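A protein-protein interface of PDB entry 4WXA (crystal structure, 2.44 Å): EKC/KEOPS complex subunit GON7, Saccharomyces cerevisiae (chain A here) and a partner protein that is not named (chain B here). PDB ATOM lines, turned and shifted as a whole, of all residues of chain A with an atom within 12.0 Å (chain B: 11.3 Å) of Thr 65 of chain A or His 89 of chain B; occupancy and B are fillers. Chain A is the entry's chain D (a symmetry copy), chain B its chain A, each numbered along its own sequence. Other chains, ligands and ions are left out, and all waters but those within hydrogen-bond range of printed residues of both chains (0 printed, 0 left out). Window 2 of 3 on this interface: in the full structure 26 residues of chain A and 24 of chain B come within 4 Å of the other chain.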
ATOM      1  N   LYS A   2       5.096  29.910  39.479  1.00  0.00           N
ATOM      2  CA  LYS A   2       4.295  29.045  40.384  1.00  0.00           C
ATOM      3  C   LYS A   2       4.427  27.583  39.956  1.00  0.00           C
ATOM      4  O   LYS A   2       4.708  27.297  38.825  1.00  0.00           O
ATOM      5  CB  LYS A   2       2.817  29.481  40.377  1.00  0.00           C
ATOM      6  CG  LYS A   2       2.522  30.714  41.222  1.00  0.00           C
ATOM      7  CD  LYS A   2       2.581  30.376  42.716  1.00  0.00           C
ATOM      8  CE  LYS A   2       2.768  31.607  43.587  1.00  0.00           C
ATOM      9  NZ  LYS A   2       1.727  32.626  43.260  1.00  0.00           N
ATOM     10  N   LEU A   3       4.246  26.653  40.874  1.00  0.00           N
ATOM     11  CA  LEU A   3       4.364  25.252  40.543  1.00  0.00           C
ATOM     12  C   LEU A   3       3.010  24.676  40.151  1.00  0.00           C
ATOM     13  O   LEU A   3       1.967  25.190  40.529  1.00  0.00           O
ATOM     14  CB  LEU A   3       4.867  24.487  41.741  1.00  0.00           C
ATOM     15  CG  LEU A   3       6.063  25.038  42.514  1.00  0.00           C
ATOM     16  CD1 LEU A   3       6.130  24.393  43.900  1.00  0.00           C
ATOM     17  CD2 LEU A   3       7.321  24.757  41.716  1.00  0.00           C
ATOM     18  N   PRO A   4       3.026  23.575  39.421  1.00  0.00           N
ATOM     19  CA  PRO A   4       1.777  22.891  39.294  1.00  0.00           C
ATOM     20  C   PRO A   4       1.320  22.355  40.641  1.00  0.00           C
ATOM     21  O   PRO A   4       2.162  21.950  41.381  1.00  0.00           O
ATOM     22  CB  PRO A   4       2.106  21.747  38.343  1.00  0.00           C
ATOM     23  CG  PRO A   4       3.547  21.506  38.524  1.00  0.00           C
ATOM     24  CD  PRO A   4       4.147  22.833  38.842  1.00  0.00           C
ATOM     25  N   LEU A  64      18.148  23.201  31.980  1.00  0.00           N
ATOM     26  CA  LEU A  64      16.773  22.770  31.751  1.00  0.00           C
ATOM     27  C   LEU A  64      15.861  24.006  31.569  1.00  0.00           C
ATOM     28  O   LEU A  64      16.108  25.046  32.179  1.00  0.00           O
ATOM     29  CB  LEU A  64      16.301  21.874  32.912  1.00  0.00           C
ATOM     30  CG  LEU A  64      15.081  20.945  32.692  1.00  0.00           C
ATOM     31  CD1 LEU A  64      15.258  19.993  31.516  1.00  0.00           C
ATOM     32  CD2 LEU A  64      14.756  20.138  33.949  1.00  0.00           C
ATOM     33  N   THR A  65      14.833  23.904  30.720  1.00  0.00           N
ATOM     34  CA  THR A  65      13.947  25.052  30.425  1.00  0.00           C
ATOM     35  C   THR A  65      12.772  25.119  31.396  1.00  0.00           C
ATOM     36  O   THR A  65      12.459  24.129  32.076  1.00  0.00           O
ATOM     37  CB  THR A  65      13.391  24.966  29.012  1.00  0.00           C
ATOM     38  OG1 THR A  65      12.691  23.738  28.848  1.00  0.00           O
ATOM     39  CG2 THR A  65      14.485  25.009  28.017  1.00  0.00           C
ATOM     40  N   TYR A  66      12.149  26.293  31.495  1.00  0.00           N
ATOM     41  CA  TYR A  66      10.901  26.476  32.232  1.00  0.00           C
ATOM     42  C   TYR A  66       9.878  25.334  31.964  1.00  0.00           C
ATOM     43  O   TYR A  66       9.338  24.728  32.916  1.00  0.00           O
ATOM     44  CB  TYR A  66      10.214  27.824  31.860  1.00  0.00           C
ATOM     45  CG  TYR A  66       8.884  28.031  32.582  1.00  0.00           C
ATOM     46  CD1 TYR A  66       7.716  27.399  32.147  1.00  0.00           C
ATOM     47  CD2 TYR A  66       8.821  28.792  33.764  1.00  0.00           C
ATOM     48  CE1 TYR A  66       6.523  27.505  32.858  1.00  0.00           C
ATOM     49  CE2 TYR A  66       7.625  28.906  34.482  1.00  0.00           C
ATOM     50  CZ  TYR A  66       6.485  28.263  34.007  1.00  0.00           C
ATOM     51  OH  TYR A  66       5.315  28.390  34.693  1.00  0.00           O
ATOM     52  N   LEU A  67       9.563  25.100  30.681  1.00  0.00           N
ATOM     53  CA  LEU A  67       8.637  24.055  30.315  1.00  0.00           C
ATOM     54  C   LEU A  67       9.183  22.642  30.581  1.00  0.00           C
ATOM     55  O   LEU A  67       8.394  21.702  30.795  1.00  0.00           O
ATOM     56  CB  LEU A  67       8.218  24.172  28.841  1.00  0.00           C
ATOM     57  CG  LEU A  67       7.366  25.360  28.407  1.00  0.00           C
ATOM     58  CD1 LEU A  67       7.393  25.544  26.886  1.00  0.00           C
ATOM     59  CD2 LEU A  67       5.970  25.184  28.833  1.00  0.00           C
ATOM     60  N   GLY A  68      10.501  22.490  30.489  1.00  0.00           N
ATOM     61  CA  GLY A  68      11.156  21.236  30.777  1.00  0.00           C
ATOM     62  C   GLY A  68      11.006  20.898  32.240  1.00  0.00           C
ATOM     63  O   GLY A  68      10.570  19.805  32.600  1.00  0.00           O
ATOM     64  N   GLN A  69      11.348  21.863  33.081  1.00  0.00           N
ATOM     65  CA  GLN A  69      11.090  21.731  34.498  1.00  0.00           C
ATOM     66  C   GLN A  69       9.610  21.434  34.711  1.00  0.00           C
ATOM     67  O   GLN A  69       9.268  20.501  35.426  1.00  0.00           O
ATOM     68  CB  GLN A  69      11.533  22.970  35.284  1.00  0.00           C
ATOM     69  CG  GLN A  69      12.923  22.842  35.926  1.00  0.00           C
ATOM     70  CD  GLN A  69      13.260  23.982  36.889  1.00  0.00           C
ATOM     71  N   LEU A  70       8.735  22.204  34.077  1.00  0.00           N
ATOM     72  CA  LEU A  70       7.299  22.024  34.277  1.00  0.00           C
ATOM     73  C   LEU A  70       6.924  20.572  34.106  1.00  0.00           C
ATOM     74  O   LEU A  70       6.211  20.023  34.937  1.00  0.00           O
ATOM     75  CB  LEU A  70       6.478  22.871  33.300  1.00  0.00           C
ATOM     76  CG  LEU A  70       4.944  22.669  33.314  1.00  0.00           C
ATOM     77  CD1 LEU A  70       4.391  22.797  34.720  1.00  0.00           C
ATOM     78  CD2 LEU A  70       4.258  23.669  32.414  1.00  0.00           C
ATOM     79  N   ARG A  71       7.452  19.963  33.055  1.00  0.00           N
ATOM     80  CA  ARG A  71       7.150  18.584  32.721  1.00  0.00           C
ATOM     81  C   ARG A  71       7.695  17.587  33.783  1.00  0.00           C
ATOM     82  O   ARG A  71       7.050  16.581  34.053  1.00  0.00           O
ATOM     83  CB  ARG A  71       7.695  18.230  31.337  1.00  0.00           C
ATOM     84  CG  ARG A  71       7.418  16.809  30.867  1.00  0.00           C
ATOM     85  CD  ARG A  71       7.536  16.650  29.347  1.00  0.00           C
ATOM     86  NE  ARG A  71       8.921  16.503  28.880  1.00  0.00           N
ATOM     87  N   THR A  72       8.853  17.852  34.369  1.00  0.00           N
ATOM     88  CA  THR A  72       9.350  16.956  35.376  1.00  0.00           C
ATOM     89  C   THR A  72       8.486  17.128  36.596  1.00  0.00           C
ATOM     90  O   THR A  72       8.050  16.130  37.199  1.00  0.00           O
ATOM     91  CB  THR A  72      10.846  17.106  35.684  1.00  0.00           C
ATOM     92  OG1 THR A  72      11.174  18.462  35.991  1.00  0.00           O
ATOM     93  CG2 THR A  72      11.659  16.644  34.488  1.00  0.00           C
ATOM     94  N   GLN A  73       8.152  18.373  36.924  1.00  0.00           N
ATOM     95  CA  GLN A  73       7.299  18.587  38.075  1.00  0.00           C
ATOM     96  C   GLN A  73       5.980  17.823  37.909  1.00  0.00           C
ATOM     97  O   GLN A  73       5.440  17.276  38.889  1.00  0.00           O
ATOM     98  CB  GLN A  73       7.024  20.052  38.292  1.00  0.00           C
ATOM     99  CG  GLN A  73       8.175  20.833  38.858  1.00  0.00           C
ATOM    100  CD  GLN A  73       8.054  22.315  38.563  1.00  0.00           C
ATOM    101  OE1 GLN A  73       7.296  22.736  37.677  1.00  0.00           O
ATOM    102  NE2 GLN A  73       8.788  23.118  39.305  1.00  0.00           N
ATOM    103  N   LEU A  74       5.445  17.778  36.693  1.00  0.00           N
ATOM    104  CA  LEU A  74       4.185  17.077  36.505  1.00  0.00           C
ATOM    105  C   LEU A  74       4.386  15.607  36.669  1.00  0.00           C
ATOM    106  O   LEU A  74       3.485  14.910  37.065  1.00  0.00           O
ATOM    107  CB  LEU A  74       3.630  17.285  35.113  1.00  0.00           C
ATOM    108  CG  LEU A  74       2.994  18.623  34.827  1.00  0.00           C
ATOM    109  CD1 LEU A  74       2.614  18.684  33.350  1.00  0.00           C
ATOM    110  CD2 LEU A  74       1.804  18.822  35.747  1.00  0.00           C
ATOM    111  N   PRO B  18       0.419  25.847  35.638  1.00  0.00           N
ATOM    112  CA  PRO B  18       0.839  27.167  35.195  1.00  0.00           C
ATOM    113  C   PRO B  18       1.712  27.141  33.983  1.00  0.00           C
ATOM    114  O   PRO B  18       2.800  26.628  34.025  1.00  0.00           O
ATOM    115  CB  PRO B  18       1.595  27.748  36.370  1.00  0.00           C
ATOM    116  CG  PRO B  18       1.463  26.780  37.461  1.00  0.00           C
ATOM    117  CD  PRO B  18       1.004  25.476  36.916  1.00  0.00           C
ATOM    118  N   PHE B  19       1.226  27.668  32.882  1.00  0.00           N
ATOM    119  CA  PHE B  19       2.081  27.810  31.714  1.00  0.00           C
ATOM    120  C   PHE B  19       2.733  29.222  31.698  1.00  0.00           C
ATOM    121  O   PHE B  19       2.429  30.078  32.494  1.00  0.00           O
ATOM    122  CB  PHE B  19       1.214  27.616  30.481  1.00  0.00           C
ATOM    123  CG  PHE B  19       0.829  26.204  30.227  1.00  0.00           C
ATOM    124  CD1 PHE B  19      -0.273  25.698  30.786  1.00  0.00           C
ATOM    125  CD2 PHE B  19       1.583  25.401  29.395  1.00  0.00           C
ATOM    126  CE1 PHE B  19      -0.649  24.392  30.543  1.00  0.00           C
ATOM    127  CE2 PHE B  19       1.221  24.104  29.132  1.00  0.00           C
ATOM    128  CZ  PHE B  19       0.083  23.593  29.712  1.00  0.00           C
ATOM    129  N   GLU B  20       3.604  29.476  30.756  1.00  0.00           N
ATOM    130  CA  GLU B  20       4.271  30.783  30.661  1.00  0.00           C
ATOM    131  C   GLU B  20       3.318  31.907  30.197  1.00  0.00           C
ATOM    132  O   GLU B  20       3.362  32.990  30.691  1.00  0.00           O
ATOM    133  CB  GLU B  20       5.464  30.697  29.707  1.00  0.00           C
ATOM    134  CG  GLU B  20       6.503  29.595  29.934  1.00  0.00           C
ATOM    135  CD  GLU B  20       7.682  29.651  28.936  1.00  0.00           C
ATOM    136  N   GLN B  24      -0.467  30.010  25.632  1.00  0.00           N
ATOM    137  CA  GLN B  24      -0.017  28.659  25.757  1.00  0.00           C
ATOM    138  C   GLN B  24      -1.106  27.828  26.483  1.00  0.00           C
ATOM    139  O   GLN B  24      -1.352  26.688  26.133  1.00  0.00           O
ATOM    140  CB  GLN B  24       1.214  28.620  26.579  1.00  0.00           C
ATOM    141  CG  GLN B  24       2.471  28.891  25.814  1.00  0.00           C
ATOM    142  CD  GLN B  24       3.753  28.737  26.663  1.00  0.00           C
ATOM    143  OE1 GLN B  24       3.713  28.570  27.886  1.00  0.00           O
ATOM    144  NE2 GLN B  24       4.883  28.767  25.994  1.00  0.00           N
ATOM    145  N   LYS B  78       1.514  16.200  29.693  1.00  0.00           N
ATOM    146  CA  LYS B  78       2.973  16.185  29.538  1.00  0.00           C
ATOM    147  C   LYS B  78       3.372  16.209  28.096  1.00  0.00           C
ATOM    148  O   LYS B  78       4.378  16.828  27.767  1.00  0.00           O
ATOM    149  CB  LYS B  78       3.614  14.982  30.190  1.00  0.00           C
ATOM    150  CG  LYS B  78       3.547  15.069  31.714  1.00  0.00           C
ATOM    151  CD  LYS B  78       4.332  13.995  32.489  1.00  0.00           C
ATOM    152  CE  LYS B  78       3.926  12.562  32.213  1.00  0.00           C
ATOM    153  NZ  LYS B  78       4.846  11.673  32.996  1.00  0.00           N
ATOM    154  N   ILE B  80       1.773  17.510  25.554  1.00  0.00           N
ATOM    155  CA  ILE B  80       1.513  18.858  25.107  1.00  0.00           C
ATOM    156  C   ILE B  80       2.573  19.819  25.631  1.00  0.00           C
ATOM    157  O   ILE B  80       2.986  20.725  24.896  1.00  0.00           O
ATOM    158  CB  ILE B  80       0.133  19.356  25.567  1.00  0.00           C
ATOM    159  CG1 ILE B  80      -1.011  18.556  24.894  1.00  0.00           C
ATOM    160  CG2 ILE B  80      -0.059  20.812  25.203  1.00  0.00           C
ATOM    161  CD1 ILE B  80      -2.339  18.770  25.596  1.00  0.00           C
ATOM    162  N   VAL B  81       3.025  19.636  26.868  1.00  0.00           N
ATOM    163  CA  VAL B  81       4.170  20.449  27.415  1.00  0.00           C
ATOM    164  C   VAL B  81       5.490  20.192  26.695  1.00  0.00           C
ATOM    165  O   VAL B  81       6.222  21.125  26.397  1.00  0.00           O
ATOM    166  CB  VAL B  81       4.341  20.242  28.938  1.00  0.00           C
ATOM    167  CG1 VAL B  81       5.567  20.933  29.474  1.00  0.00           C
ATOM    168  CG2 VAL B  81       3.126  20.780  29.667  1.00  0.00           C
ATOM    169  N   GLU B  82       5.799  18.941  26.380  1.00  0.00           N
ATOM    170  CA  GLU B  82       7.006  18.624  25.617  1.00  0.00           C
ATOM    171  C   GLU B  82       6.936  19.374  24.269  1.00  0.00           C
ATOM    172  O   GLU B  82       7.837  20.106  23.928  1.00  0.00           O
ATOM    173  CB  GLU B  82       7.129  17.106  25.427  1.00  0.00           C
ATOM    174  CG  GLU B  82       8.484  16.568  24.959  1.00  0.00           C
ATOM    175  N   ALA B  83       5.839  19.217  23.533  1.00  0.00           N
ATOM    176  CA  ALA B  83       5.691  19.805  22.198  1.00  0.00           C
ATOM    177  C   ALA B  83       5.851  21.296  22.257  1.00  0.00           C
ATOM    178  O   ALA B  83       6.493  21.887  21.429  1.00  0.00           O
ATOM    179  CB  ALA B  83       4.311  19.486  21.619  1.00  0.00           C
ATOM    180  N   MET B  84       5.246  21.913  23.244  1.00  0.00           N
ATOM    181  CA  MET B  84       5.390  23.348  23.412  1.00  0.00           C
ATOM    182  C   MET B  84       6.814  23.796  23.729  1.00  0.00           C
ATOM    183  O   MET B  84       7.255  24.834  23.247  1.00  0.00           O
ATOM    184  CB  MET B  84       4.445  23.830  24.501  1.00  0.00           C
ATOM    185  CG  MET B  84       3.228  24.457  23.910  1.00  0.00           C
ATOM    186  SD  MET B  84       1.974  24.758  25.110  1.00  0.00           S
ATOM    187  CE  MET B  84       0.673  25.144  23.965  1.00  0.00           C
ATOM    188  N   ASP B  85       7.523  23.010  24.543  1.00  0.00           N
ATOM    189  CA  ASP B  85       8.954  23.200  24.814  1.00  0.00           C
ATOM    190  C   ASP B  85       9.784  23.204  23.517  1.00  0.00           C
ATOM    191  O   ASP B  85      10.671  24.032  23.326  1.00  0.00           O
ATOM    192  CB  ASP B  85       9.419  22.050  25.746  1.00  0.00           C
ATOM    193  CG  ASP B  85      10.758  22.303  26.446  1.00  0.00           C
ATOM    194  OD1 ASP B  85      11.412  23.362  26.280  1.00  0.00           O
ATOM    195  OD2 ASP B  85      11.157  21.374  27.199  1.00  0.00           O
ATOM    196  N   VAL B  86       9.512  22.254  22.639  1.00  0.00           N
ATOM    197  CA  VAL B  86      10.242  22.161  21.397  1.00  0.00           C
ATOM    198  C   VAL B  86       9.958  23.428  20.539  1.00  0.00           C
ATOM    199  O   VAL B  86      10.868  24.107  20.108  1.00  0.00           O
ATOM    200  CB  VAL B  86       9.827  20.873  20.651  1.00  0.00           C
ATOM    201  CG1 VAL B  86      10.264  20.896  19.196  1.00  0.00           C
ATOM    202  CG2 VAL B  86      10.381  19.645  21.338  1.00  0.00           C
ATOM    203  N   LEU B  87       8.692  23.752  20.341  1.00  0.00           N
ATOM    204  CA  LEU B  87       8.313  24.834  19.473  1.00  0.00           C
ATOM    205  C   LEU B  87       8.766  26.228  19.911  1.00  0.00           C
ATOM    206  O   LEU B  87       9.197  26.997  19.072  1.00  0.00           O
ATOM    207  CB  LEU B  87       6.795  24.851  19.271  1.00  0.00           C
ATOM    208  CG  LEU B  87       6.261  23.713  18.412  1.00  0.00           C
ATOM    209  CD1 LEU B  87       4.744  23.774  18.373  1.00  0.00           C
ATOM    210  CD2 LEU B  87       6.840  23.826  17.019  1.00  0.00           C
ATOM    211  N   SER B  88       8.670  26.543  21.199  1.00  0.00           N
ATOM    212  CA  SER B  88       9.035  27.859  21.697  1.00  0.00           C
ATOM    213  C   SER B  88      10.537  28.126  21.696  1.00  0.00           C
ATOM    214  O   SER B  88      10.951  29.251  21.882  1.00  0.00           O
ATOM    215  CB  SER B  88       8.432  28.114  23.091  1.00  0.00           C
ATOM    216  OG  SER B  88       8.709  27.096  24.040  1.00  0.00           O
ATOM    217  N   HIS B  89      11.344  27.110  21.440  1.00  0.00           N
ATOM    218  CA  HIS B  89      12.784  27.265  21.481  1.00  0.00           C
ATOM    219  C   HIS B  89      13.344  27.165  20.102  1.00  0.00           C
ATOM    220  O   HIS B  89      14.476  26.828  19.930  1.00  0.00           O
ATOM    221  CB  HIS B  89      13.423  26.262  22.468  1.00  0.00           C
ATOM    222  CG  HIS B  89      13.141  26.592  23.907  1.00  0.00           C
ATOM    223  ND1 HIS B  89      12.146  25.976  24.647  1.00  0.00           N
ATOM    224  CD2 HIS B  89      13.711  27.503  24.736  1.00  0.00           C
ATOM    225  CE1 HIS B  89      12.115  26.498  25.866  1.00  0.00           C
ATOM    226  NE2 HIS B  89      13.058  27.424  25.945  1.00  0.00           N
ATOM    227  N   HIS B  90      12.561  27.532  19.101  1.00  0.00           N
ATOM    228  CA  HIS B  90      13.129  27.799  17.774  1.00  0.00           C
ATOM    229  C   HIS B  90      12.439  29.010  17.085  1.00  0.00           C
ATOM    230  O   HIS B  90      11.418  29.563  17.577  1.00  0.00           O
ATOM    231  CB  HIS B  90      13.083  26.494  16.947  1.00  0.00           C
ATOM    232  CG  HIS B  90      13.872  25.353  17.546  1.00  0.00           C
ATOM    233  ND1 HIS B  90      13.382  24.539  18.558  1.00  0.00           N
ATOM    234  CD2 HIS B  90      15.121  24.894  17.275  1.00  0.00           C
ATOM    235  CE1 HIS B  90      14.290  23.631  18.878  1.00  0.00           C
ATOM    236  NE2 HIS B  90      15.356  23.827  18.118  1.00  0.00           N
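The backbone carbonyl oxygen (O) of Pro 18 of chain B is in hydrogen-bond range of the side-chain hydroxyl (OH) of Tyr 66 of chain A (3.1 Å). The side-chain carboxylate of Asp 85 of chain B is in hydrogen-bond range of the side-chain hydroxyl of Thr 65 of chain A.
The backbone NH (N) of Glu 20 of chain B sits at hydrogen-bond distance from the side-chain amide oxygen (OE1) of Gln 24 of chain B (3.0 Å). O of Met 84 of chain B sits at hydrogen-bond distance from OG of Ser 88 of chain B, 2.8 Å away. ND1 of His 89 of chain B sits at hydrogen-bond distance from O of Asp 85 of chain B (2.8 Å). OG1 of Thr 65 of chain A sits at hydrogen-bond distance from N of Gly 68 of chain A (3.0 Å).
Among the printed residues, pairs that only touch across the chains: Lys 2 of chain A with Pro 18 of chain B (3.6 Å), Leu 3 of chain A with Pro 18 of chain B (3.5 Å), Pro 4 of chain A with Pro 18 of chain B (3.6 Å), Thr 65 of chain A with His 89 of chain B (3.5 Å), Tyr 66 of chain A with Glu 20 of chain B (3.3 Å), Leu 67 of chain A with Val 81 of chain B (3.2 Å), Leu 67 of chain A with Met 84 of chain B (3.7 Å), Leu 67 of chain A with Asp 85 of chain B (3.5 Å), Leu 67 of chain A with Ser 88 of chain B (3.5 Å), Gly 68 of chain A with Asp 85 of chain B (3.5 Å), Leu 70 of chain A with Pro 18 of chain B (3.7 Å), Arg 71 of chain A with Lys 78 of chain B (3.5 Å), Arg 71 of chain A with Val 81 of chain B (3.9 Å) and Arg 71 of chain A with Glu 82 of chain B (3.9 Å).
Thr 65 of chain A touches two residues of chain B. Of chain A, only Thr 65 comes within 4 Å of His 89 of chain B. Of the printed residues of chain B, Gly 68 of chain A touches Asp 85 (3.5 Å). No residue of chain B comes within 4 Å of Gln 69 of chain A. Asp 85 of chain B touches just these residues of chain A: Thr 65, Leu 67 and Gly 68. Of chain A, only Leu 67 comes within 4 Å of Ser 88 of chain B. No residue of chain A comes within 4 Å of His 90 of chain B. Of the printed residues of chain A, Lys 78 of chain B touches Arg 71. Printed residues of chain B within 4 Å of Leu 3 of chain A: Pro 18 (3.5 Å). Of the printed residues of chain B, Leu 70 of chain A touches Pro 18. Of the printed residues of chain B, Lys 2 of chain A touches Pro 18 (3.6 Å). Printed residues of chain A within 4 Å of Glu 20 of chain B: Tyr 66. Gln 24 of chain B touches none of the printed residues of chain A.
Hydrophobic or aromatic side chains of chain A that line the printed part of chain B: Tyr 66, Leu 67 and Leu 70. Hydrophobic or aromatic side chains of chain B within 4 Å of the printed part of chain A: Pro 18, Val 81 and His 89.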
